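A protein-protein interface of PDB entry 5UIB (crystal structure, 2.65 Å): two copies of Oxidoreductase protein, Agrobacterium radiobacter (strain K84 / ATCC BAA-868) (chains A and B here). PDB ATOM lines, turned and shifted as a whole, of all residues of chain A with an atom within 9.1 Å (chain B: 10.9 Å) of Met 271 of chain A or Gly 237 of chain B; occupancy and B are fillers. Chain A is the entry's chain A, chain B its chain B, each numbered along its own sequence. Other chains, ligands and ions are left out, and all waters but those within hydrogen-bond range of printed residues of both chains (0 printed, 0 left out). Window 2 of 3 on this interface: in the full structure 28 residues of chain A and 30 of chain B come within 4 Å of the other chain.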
ATOM      1  N   GLY A 253     -33.229 -23.648  -7.946  1.00  0.00           N
ATOM      2  CA  GLY A 253     -32.099 -24.139  -7.151  1.00  0.00           C
ATOM      3  C   GLY A 253     -31.746 -23.381  -5.878  1.00  0.00           C
ATOM      4  O   GLY A 253     -32.478 -22.490  -5.447  1.00  0.00           O
ATOM      5  N   THR A 254     -30.598 -23.735  -5.295  1.00  0.00           N
ATOM      6  CA  THR A 254     -30.123 -23.175  -4.020  1.00  0.00           C
ATOM      7  C   THR A 254     -28.613 -22.896  -4.041  1.00  0.00           C
ATOM      8  O   THR A 254     -27.845 -23.660  -4.635  1.00  0.00           O
ATOM      9  CB  THR A 254     -30.413 -24.130  -2.827  1.00  0.00           C
ATOM     10  OG1 THR A 254     -29.856 -25.425  -3.087  1.00  0.00           O
ATOM     11  CG2 THR A 254     -31.925 -24.278  -2.566  1.00  0.00           C
ATOM     12  N   ILE A 255     -28.209 -21.790  -3.406  1.00  0.00           N
ATOM     13  CA  ILE A 255     -26.795 -21.459  -3.143  1.00  0.00           C
ATOM     14  C   ILE A 255     -26.571 -21.585  -1.641  1.00  0.00           C
ATOM     15  O   ILE A 255     -27.445 -21.221  -0.857  1.00  0.00           O
ATOM     16  CB  ILE A 255     -26.429 -20.017  -3.568  1.00  0.00           C
ATOM     17  CG1 ILE A 255     -26.712 -19.803  -5.062  1.00  0.00           C
ATOM     18  CG2 ILE A 255     -24.962 -19.712  -3.243  1.00  0.00           C
ATOM     19  CD1 ILE A 255     -26.662 -18.349  -5.500  1.00  0.00           C
ATOM     20  N   ARG A 256     -25.407 -22.098  -1.242  1.00  0.00           N
ATOM     21  CA  ARG A 256     -25.059 -22.262   0.180  1.00  0.00           C
ATOM     22  C   ARG A 256     -23.568 -21.986   0.416  1.00  0.00           C
ATOM     23  O   ARG A 256     -22.731 -22.896   0.326  1.00  0.00           O
ATOM     24  CB  ARG A 256     -25.441 -23.670   0.681  1.00  0.00           C
ATOM     25  CG  ARG A 256     -26.939 -23.955   0.737  1.00  0.00           C
ATOM     26  CD  ARG A 256     -27.620 -23.084   1.778  1.00  0.00           C
ATOM     27  NE  ARG A 256     -29.023 -23.427   1.979  1.00  0.00           N
ATOM     28  CZ  ARG A 256     -30.050 -23.022   1.225  1.00  0.00           C
ATOM     29  NH1 ARG A 256     -29.876 -22.235   0.163  1.00  0.00           N
ATOM     30  NH2 ARG A 256     -31.283 -23.418   1.540  1.00  0.00           N
ATOM     31  N   LEU A 263     -18.629 -23.410  -1.203  1.00  0.00           N
ATOM     32  CA  LEU A 263     -19.770 -22.847  -1.937  1.00  0.00           C
ATOM     33  C   LEU A 263     -20.547 -23.948  -2.664  1.00  0.00           C
ATOM     34  O   LEU A 263     -20.079 -24.457  -3.677  1.00  0.00           O
ATOM     35  CB  LEU A 263     -19.263 -21.813  -2.939  1.00  0.00           C
ATOM     36  CG  LEU A 263     -20.283 -21.209  -3.895  1.00  0.00           C
ATOM     37  CD1 LEU A 263     -21.352 -20.465  -3.106  1.00  0.00           C
ATOM     38  CD2 LEU A 263     -19.588 -20.295  -4.897  1.00  0.00           C
ATOM     39  N   GLU A 264     -21.722 -24.315  -2.147  1.00  0.00           N
ATOM     40  CA  GLU A 264     -22.554 -25.358  -2.758  1.00  0.00           C
ATOM     41  C   GLU A 264     -23.631 -24.701  -3.612  1.00  0.00           C
ATOM     42  O   GLU A 264     -24.363 -23.847  -3.137  1.00  0.00           O
ATOM     43  CB  GLU A 264     -23.193 -26.252  -1.689  1.00  0.00           C
ATOM     44  CG  GLU A 264     -22.272 -27.320  -1.100  1.00  0.00           C
ATOM     45  CD  GLU A 264     -22.902 -28.082   0.081  1.00  0.00           C
ATOM     46  OE1 GLU A 264     -24.140 -28.306   0.068  1.00  0.00           O
ATOM     47  OE2 GLU A 264     -22.164 -28.467   1.025  1.00  0.00           O
ATOM     48  N   VAL A 265     -23.704 -25.082  -4.878  1.00  0.00           N
ATOM     49  CA  VAL A 265     -24.768 -24.630  -5.769  1.00  0.00           C
ATOM     50  C   VAL A 265     -25.461 -25.873  -6.304  1.00  0.00           C
ATOM     51  O   VAL A 265     -24.789 -26.831  -6.704  1.00  0.00           O
ATOM     52  CB  VAL A 265     -24.225 -23.808  -6.960  1.00  0.00           C
ATOM     53  CG1 VAL A 265     -25.365 -23.352  -7.874  1.00  0.00           C
ATOM     54  CG2 VAL A 265     -23.416 -22.615  -6.463  1.00  0.00           C
ATOM     55  N   THR A 266     -26.792 -25.863  -6.312  1.00  0.00           N
ATOM     56  CA  THR A 266     -27.563 -26.981  -6.843  1.00  0.00           C
ATOM     57  C   THR A 266     -28.612 -26.449  -7.805  1.00  0.00           C
ATOM     58  O   THR A 266     -29.312 -25.496  -7.493  1.00  0.00           O
ATOM     59  CB  THR A 266     -28.169 -27.837  -5.710  1.00  0.00           C
ATOM     60  OG1 THR A 266     -27.118 -28.595  -5.098  1.00  0.00           O
ATOM     61  CG2 THR A 266     -29.227 -28.822  -6.225  1.00  0.00           C
ATOM     62  N   GLY A 267     -28.683 -27.066  -8.981  1.00  0.00           N
ATOM     63  CA  GLY A 267     -29.617 -26.678 -10.032  1.00  0.00           C
ATOM     64  C   GLY A 267     -30.089 -27.893 -10.814  1.00  0.00           C
ATOM     65  O   GLY A 267     -29.921 -29.029 -10.359  1.00  0.00           O
ATOM     66  N   PRO A 268     -30.702 -27.662 -11.989  1.00  0.00           N
ATOM     67  CA  PRO A 268     -31.141 -28.739 -12.881  1.00  0.00           C
ATOM     68  C   PRO A 268     -30.064 -29.797 -13.214  1.00  0.00           C
ATOM     69  O   PRO A 268     -30.348 -30.996 -13.120  1.00  0.00           O
ATOM     70  CB  PRO A 268     -31.571 -27.981 -14.141  1.00  0.00           C
ATOM     71  CG  PRO A 268     -32.058 -26.673 -13.623  1.00  0.00           C
ATOM     72  CD  PRO A 268     -31.194 -26.345 -12.441  1.00  0.00           C
ATOM     73  N   ASN A 269     -28.857 -29.352 -13.585  1.00  0.00           N
ATOM     74  CA  ASN A 269     -27.729 -30.254 -13.915  1.00  0.00           C
ATOM     75  C   ASN A 269     -27.229 -31.055 -12.700  1.00  0.00           C
ATOM     76  O   ASN A 269     -26.838 -32.221 -12.844  1.00  0.00           O
ATOM     77  CB  ASN A 269     -26.558 -29.474 -14.527  1.00  0.00           C
ATOM     78  N   GLY A 270     -27.235 -30.424 -11.520  1.00  0.00           N
ATOM     79  CA  GLY A 270     -26.925 -31.099 -10.247  1.00  0.00           C
ATOM     80  C   GLY A 270     -26.246 -30.191  -9.235  1.00  0.00           C
ATOM     81  O   GLY A 270     -26.392 -28.976  -9.286  1.00  0.00           O
ATOM     82  N   MET A 271     -25.502 -30.796  -8.316  1.00  0.00           N
ATOM     83  CA  MET A 271     -24.724 -30.063  -7.327  1.00  0.00           C
ATOM     84  C   MET A 271     -23.311 -29.777  -7.855  1.00  0.00           C
ATOM     85  O   MET A 271     -22.753 -30.560  -8.631  1.00  0.00           O
ATOM     86  CB  MET A 271     -24.647 -30.873  -6.029  1.00  0.00           C
ATOM     87  CG  MET A 271     -23.842 -30.230  -4.905  1.00  0.00           C
ATOM     88  SD  MET A 271     -24.164 -30.928  -3.264  1.00  0.00           S
ATOM     89  CE  MET A 271     -24.472 -32.665  -3.609  1.00  0.00           C
ATOM     90  N   THR A 272     -22.747 -28.644  -7.432  1.00  0.00           N
ATOM     91  CA  THR A 272     -21.318 -28.341  -7.610  1.00  0.00           C
ATOM     92  C   THR A 272     -20.751 -27.748  -6.311  1.00  0.00           C
ATOM     93  O   THR A 272     -21.380 -26.883  -5.712  1.00  0.00           O
ATOM     94  CB  THR A 272     -21.089 -27.364  -8.779  1.00  0.00           C
ATOM     95  OG1 THR A 272     -21.888 -26.192  -8.591  1.00  0.00           O
ATOM     96  CG2 THR A 272     -21.468 -28.012 -10.099  1.00  0.00           C
ATOM     97  N   ILE A 273     -19.596 -28.240  -5.862  1.00  0.00           N
ATOM     98  CA  ILE A 273     -18.912 -27.695  -4.687  1.00  0.00           C
ATOM     99  C   ILE A 273     -17.677 -26.973  -5.178  1.00  0.00           C
ATOM    100  O   ILE A 273     -16.837 -27.569  -5.836  1.00  0.00           O
ATOM    101  CB  ILE A 273     -18.439 -28.781  -3.696  1.00  0.00           C
ATOM    102  CG1 ILE A 273     -19.608 -29.649  -3.202  1.00  0.00           C
ATOM    103  CG2 ILE A 273     -17.717 -28.143  -2.504  1.00  0.00           C
ATOM    104  CD1 ILE A 273     -19.165 -31.015  -2.708  1.00  0.00           C
ATOM    105  N   SER A 274     -17.557 -25.707  -4.807  1.00  0.00           N
ATOM    106  CA  SER A 274     -16.503 -24.837  -5.295  1.00  0.00           C
ATOM    107  C   SER A 274     -15.781 -24.177  -4.110  1.00  0.00           C
ATOM    108  O   SER A 274     -16.395 -23.842  -3.096  1.00  0.00           O
ATOM    109  CB  SER A 274     -17.117 -23.787  -6.220  1.00  0.00           C
ATOM    110  OG  SER A 274     -18.240 -24.322  -6.909  1.00  0.00           O
ATOM    111  N   ARG B 156     -36.323 -26.651   5.687  1.00  0.00           N
ATOM    112  CA  ARG B 156     -36.272 -26.233   4.281  1.00  0.00           C
ATOM    113  C   ARG B 156     -36.075 -27.473   3.421  1.00  0.00           C
ATOM    114  O   ARG B 156     -35.003 -28.075   3.433  1.00  0.00           O
ATOM    115  CB  ARG B 156     -35.142 -25.218   4.046  1.00  0.00           C
ATOM    116  CG  ARG B 156     -35.195 -23.982   4.936  1.00  0.00           C
ATOM    117  CD  ARG B 156     -34.252 -22.898   4.441  1.00  0.00           C
ATOM    118  NE  ARG B 156     -34.803 -22.244   3.253  1.00  0.00           N
ATOM    119  CZ  ARG B 156     -35.798 -21.350   3.250  1.00  0.00           C
ATOM    120  NH1 ARG B 156     -36.381 -20.946   4.387  1.00  0.00           N
ATOM    121  NH2 ARG B 156     -36.223 -20.855   2.090  1.00  0.00           N
ATOM    122  N   SER B 157     -37.115 -27.841   2.678  1.00  0.00           N
ATOM    123  CA  SER B 157     -37.173 -29.104   1.947  1.00  0.00           C
ATOM    124  C   SER B 157     -37.753 -28.888   0.548  1.00  0.00           C
ATOM    125  O   SER B 157     -38.439 -27.898   0.313  1.00  0.00           O
ATOM    126  CB  SER B 157     -38.047 -30.074   2.744  1.00  0.00           C
ATOM    127  OG  SER B 157     -38.458 -31.190   1.978  1.00  0.00           O
ATOM    128  N   GLY B 158     -37.438 -29.797  -0.378  1.00  0.00           N
ATOM    129  CA  GLY B 158     -38.118 -29.892  -1.682  1.00  0.00           C
ATOM    130  C   GLY B 158     -38.857 -31.207  -1.869  1.00  0.00           C
ATOM    131  O   GLY B 158     -39.105 -31.641  -2.997  1.00  0.00           O
ATOM    132  N   PHE B 159     -39.231 -31.832  -0.756  1.00  0.00           N
ATOM    133  CA  PHE B 159     -39.821 -33.175  -0.755  1.00  0.00           C
ATOM    134  C   PHE B 159     -41.247 -33.115  -1.276  1.00  0.00           C
ATOM    135  O   PHE B 159     -41.971 -32.154  -1.001  1.00  0.00           O
ATOM    136  CB  PHE B 159     -39.811 -33.775   0.664  1.00  0.00           C
ATOM    137  CG  PHE B 159     -40.203 -35.224   0.712  1.00  0.00           C
ATOM    138  CD1 PHE B 159     -39.255 -36.224   0.490  1.00  0.00           C
ATOM    139  CD2 PHE B 159     -41.523 -35.596   0.959  1.00  0.00           C
ATOM    140  CE1 PHE B 159     -39.616 -37.563   0.522  1.00  0.00           C
ATOM    141  CE2 PHE B 159     -41.886 -36.933   0.988  1.00  0.00           C
ATOM    142  CZ  PHE B 159     -40.935 -37.917   0.771  1.00  0.00           C
ATOM    143  N   ALA B 233     -40.450 -25.322  -1.189  1.00  0.00           N
ATOM    144  CA  ALA B 233     -39.966 -24.988  -2.536  1.00  0.00           C
ATOM    145  C   ALA B 233     -38.453 -24.760  -2.520  1.00  0.00           C
ATOM    146  O   ALA B 233     -37.964 -23.844  -3.161  1.00  0.00           O
ATOM    147  CB  ALA B 233     -40.678 -23.749  -3.051  1.00  0.00           C
ATOM    148  N   THR B 234     -37.723 -25.628  -1.815  1.00  0.00           N
ATOM    149  CA  THR B 234     -36.270 -25.507  -1.594  1.00  0.00           C
ATOM    150  C   THR B 234     -35.518 -26.742  -2.121  1.00  0.00           C
ATOM    151  O   THR B 234     -35.618 -27.833  -1.566  1.00  0.00           O
ATOM    152  CB  THR B 234     -35.966 -25.295  -0.090  1.00  0.00           C
ATOM    153  OG1 THR B 234     -36.476 -24.022   0.325  1.00  0.00           O
ATOM    154  CG2 THR B 234     -34.456 -25.344   0.207  1.00  0.00           C
ATOM    155  N   LYS B 235     -34.726 -26.539  -3.166  1.00  0.00           N
ATOM    156  CA  LYS B 235     -34.101 -27.632  -3.894  1.00  0.00           C
ATOM    157  C   LYS B 235     -32.627 -27.791  -3.524  1.00  0.00           C
ATOM    158  O   LYS B 235     -31.761 -27.111  -4.061  1.00  0.00           O
ATOM    159  CB  LYS B 235     -34.296 -27.400  -5.389  1.00  0.00           C
ATOM    160  CG  LYS B 235     -35.751 -27.076  -5.732  1.00  0.00           C
ATOM    161  CD  LYS B 235     -36.147 -27.542  -7.123  1.00  0.00           C
ATOM    162  CE  LYS B 235     -37.657 -27.550  -7.327  1.00  0.00           C
ATOM    163  NZ  LYS B 235     -38.150 -26.199  -7.704  1.00  0.00           N
ATOM    164  N   LEU B 236     -32.362 -28.706  -2.594  1.00  0.00           N
ATOM    165  CA  LEU B 236     -31.010 -28.957  -2.093  1.00  0.00           C
ATOM    166  C   LEU B 236     -30.388 -30.216  -2.692  1.00  0.00           C
ATOM    167  O   LEU B 236     -31.088 -31.162  -3.049  1.00  0.00           O
ATOM    168  CB  LEU B 236     -31.035 -29.079  -0.569  1.00  0.00           C
ATOM    169  CG  LEU B 236     -31.364 -27.780   0.174  1.00  0.00           C
ATOM    170  CD1 LEU B 236     -31.897 -28.071   1.570  1.00  0.00           C
ATOM    171  CD2 LEU B 236     -30.149 -26.863   0.232  1.00  0.00           C
ATOM    172  N   GLY B 237     -29.061 -30.217  -2.772  1.00  0.00           N
ATOM    173  CA  GLY B 237     -28.302 -31.347  -3.294  1.00  0.00           C
ATOM    174  C   GLY B 237     -28.401 -32.617  -2.466  1.00  0.00           C
ATOM    175  O   GLY B 237     -28.177 -33.704  -2.988  1.00  0.00           O
ATOM    176  N   THR B 238     -28.703 -32.476  -1.174  1.00  0.00           N
ATOM    177  CA  THR B 238     -29.053 -33.611  -0.304  1.00  0.00           C
ATOM    178  C   THR B 238     -30.306 -33.232   0.477  1.00  0.00           C
ATOM    179  O   THR B 238     -30.276 -32.303   1.282  1.00  0.00           O
ATOM    180  CB  THR B 238     -27.910 -33.981   0.670  1.00  0.00           C
ATOM    181  OG1 THR B 238     -26.637 -33.803   0.025  1.00  0.00           O
ATOM    182  CG2 THR B 238     -28.052 -35.426   1.122  1.00  0.00           C
ATOM    183  N   GLU B 239     -31.396 -33.952   0.217  1.00  0.00           N
ATOM    184  CA  GLU B 239     -32.732 -33.613   0.726  1.00  0.00           C
ATOM    185  C   GLU B 239     -32.849 -33.852   2.246  1.00  0.00           C
ATOM    186  O   GLU B 239     -32.847 -35.002   2.680  1.00  0.00           O
ATOM    187  CB  GLU B 239     -33.801 -34.426  -0.039  1.00  0.00           C
ATOM    188  CG  GLU B 239     -35.242 -34.269   0.444  1.00  0.00           C
ATOM    189  CD  GLU B 239     -35.691 -32.819   0.542  1.00  0.00           C
ATOM    190  OE1 GLU B 239     -35.785 -32.146  -0.515  1.00  0.00           O
ATOM    191  OE2 GLU B 239     -35.960 -32.342   1.670  1.00  0.00           O
ATOM    192  N   PRO B 240     -32.979 -32.771   3.053  1.00  0.00           N
ATOM    193  CA  PRO B 240     -32.994 -32.949   4.510  1.00  0.00           C
ATOM    194  C   PRO B 240     -34.284 -33.528   5.116  1.00  0.00           C
ATOM    195  O   PRO B 240     -34.273 -33.916   6.276  1.00  0.00           O
ATOM    196  CB  PRO B 240     -32.769 -31.525   5.030  1.00  0.00           C
ATOM    197  CG  PRO B 240     -33.386 -30.663   3.993  1.00  0.00           C
ATOM    198  CD  PRO B 240     -33.082 -31.340   2.691  1.00  0.00           C
ATOM    199  N   PHE B 241     -35.370 -33.580   4.356  1.00  0.00           N
ATOM    200  CA  PHE B 241     -36.662 -34.025   4.870  1.00  0.00           C
ATOM    201  C   PHE B 241     -36.570 -35.333   5.685  1.00  0.00           C
ATOM    202  O   PHE B 241     -35.905 -36.268   5.231  1.00  0.00           O
ATOM    203  CB  PHE B 241     -37.619 -34.214   3.695  1.00  0.00           C
ATOM    204  CG  PHE B 241     -38.980 -34.670   4.090  1.00  0.00           C
ATOM    205  CD1 PHE B 241     -39.884 -33.776   4.638  1.00  0.00           C
ATOM    206  CD2 PHE B 241     -39.365 -35.997   3.913  1.00  0.00           C
ATOM    207  CE1 PHE B 241     -41.156 -34.195   5.002  1.00  0.00           C
ATOM    208  CE2 PHE B 241     -40.631 -36.430   4.283  1.00  0.00           C
ATOM    209  CZ  PHE B 241     -41.530 -35.526   4.829  1.00  0.00           C
ATOM    210  N   GLN B 259     -27.733 -31.082   9.541  1.00  0.00           N
ATOM    211  CA  GLN B 259     -28.230 -32.235   8.763  1.00  0.00           C
ATOM    212  C   GLN B 259     -27.530 -33.555   9.148  1.00  0.00           C
ATOM    213  O   GLN B 259     -26.359 -33.556   9.504  1.00  0.00           O
ATOM    214  CB  GLN B 259     -28.093 -31.989   7.249  1.00  0.00           C
ATOM    215  CG  GLN B 259     -29.116 -32.747   6.396  1.00  0.00           C
ATOM    216  CD  GLN B 259     -28.578 -33.180   5.033  1.00  0.00           C
ATOM    217  OE1 GLN B 259     -28.011 -32.373   4.272  1.00  0.00           O
ATOM    218  NE2 GLN B 259     -28.758 -34.463   4.712  1.00  0.00           N
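OG1 of Thr 254 of chain A is in hydrogen-bond range of O of Lys 235 of chain B, at 2.7 Å.
OG1 of Thr 266 of chain A is in hydrogen-bond range of N of Gly 237 of chain B, at 3.4 Å.
The backbone carbonyl oxygen (O) of Thr 254 of chain A lies within hydrogen-bond range of the backbone NH (N) of Thr 266 of chain A, at 3.0 Å.
O of Glu 264 of chain A is in hydrogen-bond range of N of Arg 256 of chain A (2.8 Å).
O of Ser 157 of chain B is in hydrogen-bond range of N of Thr 234 of chain B.
N of Gly 158 of chain B is in hydrogen-bond range of O of Thr 234 of chain B (2.9 Å).
CG2 of Thr 234 of chain B touches CG2 of Thr 254 of chain A (3.9 Å).
Leu 236 of chain B touches Thr 254 of chain A (CD2 to OG1, 3.6 Å).
Thr 234 of chain B touches Arg 256 of chain A.
Arg 256 of chain A touches Leu 236 of chain B.
Lys 235 of chain B touches Thr 266 of chain A (O to CG2, 3.7 Å).
Thr 266 of chain A touches Leu 236 of chain B (CG2 to C, 3.97 Å).
Met 271 of chain A touches Gly 237 of chain B (CE to O, 3.9 Å).
Leu 263 of chain A touches none of the printed residues of chain B.
Of chain B, only Lys 235, Leu 236 and Gly 237 come within 4 Å of Thr 266 of chain A.
No residue of chain B comes within 4 Å of Gly 267 of chain A.
No residue of chain B comes within 4 Å of Asn 269 of chain A.
Met 271 of chain A touches one residue of chain B.
Printed residues of chain A within 4 Å of Thr 234 of chain B: Thr 254 and Arg 256.
Of the printed residues of chain A, Leu 236 of chain B touches Thr 254, Arg 256 and Thr 266.
Of chain A, only Thr 266 and Met 271 come within 4 Å of Gly 237 of chain B.
No residue of chain A comes within 4 Å of Thr 238 of chain B.
Gln 259 of chain B touches none of the printed residues of chain A.
The nearest residue of chain B that does not touch Met 271 of chain A is Thr 238 of chain B (4.4 Å).
The nearest printed residue of chain A that does not touch Thr 234 of chain B is Gly 253 of chain A (6.2 Å).
Of the 16 printed residues of chain A, 4 touch a printed residue of chain B.
Among the printed residues, 9 pairs touch across the chains.
No position is printed for both chains.
Of the 9 pairs that touch across the chains among the printed residues, none has its exchanged pair printed and touching as well.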
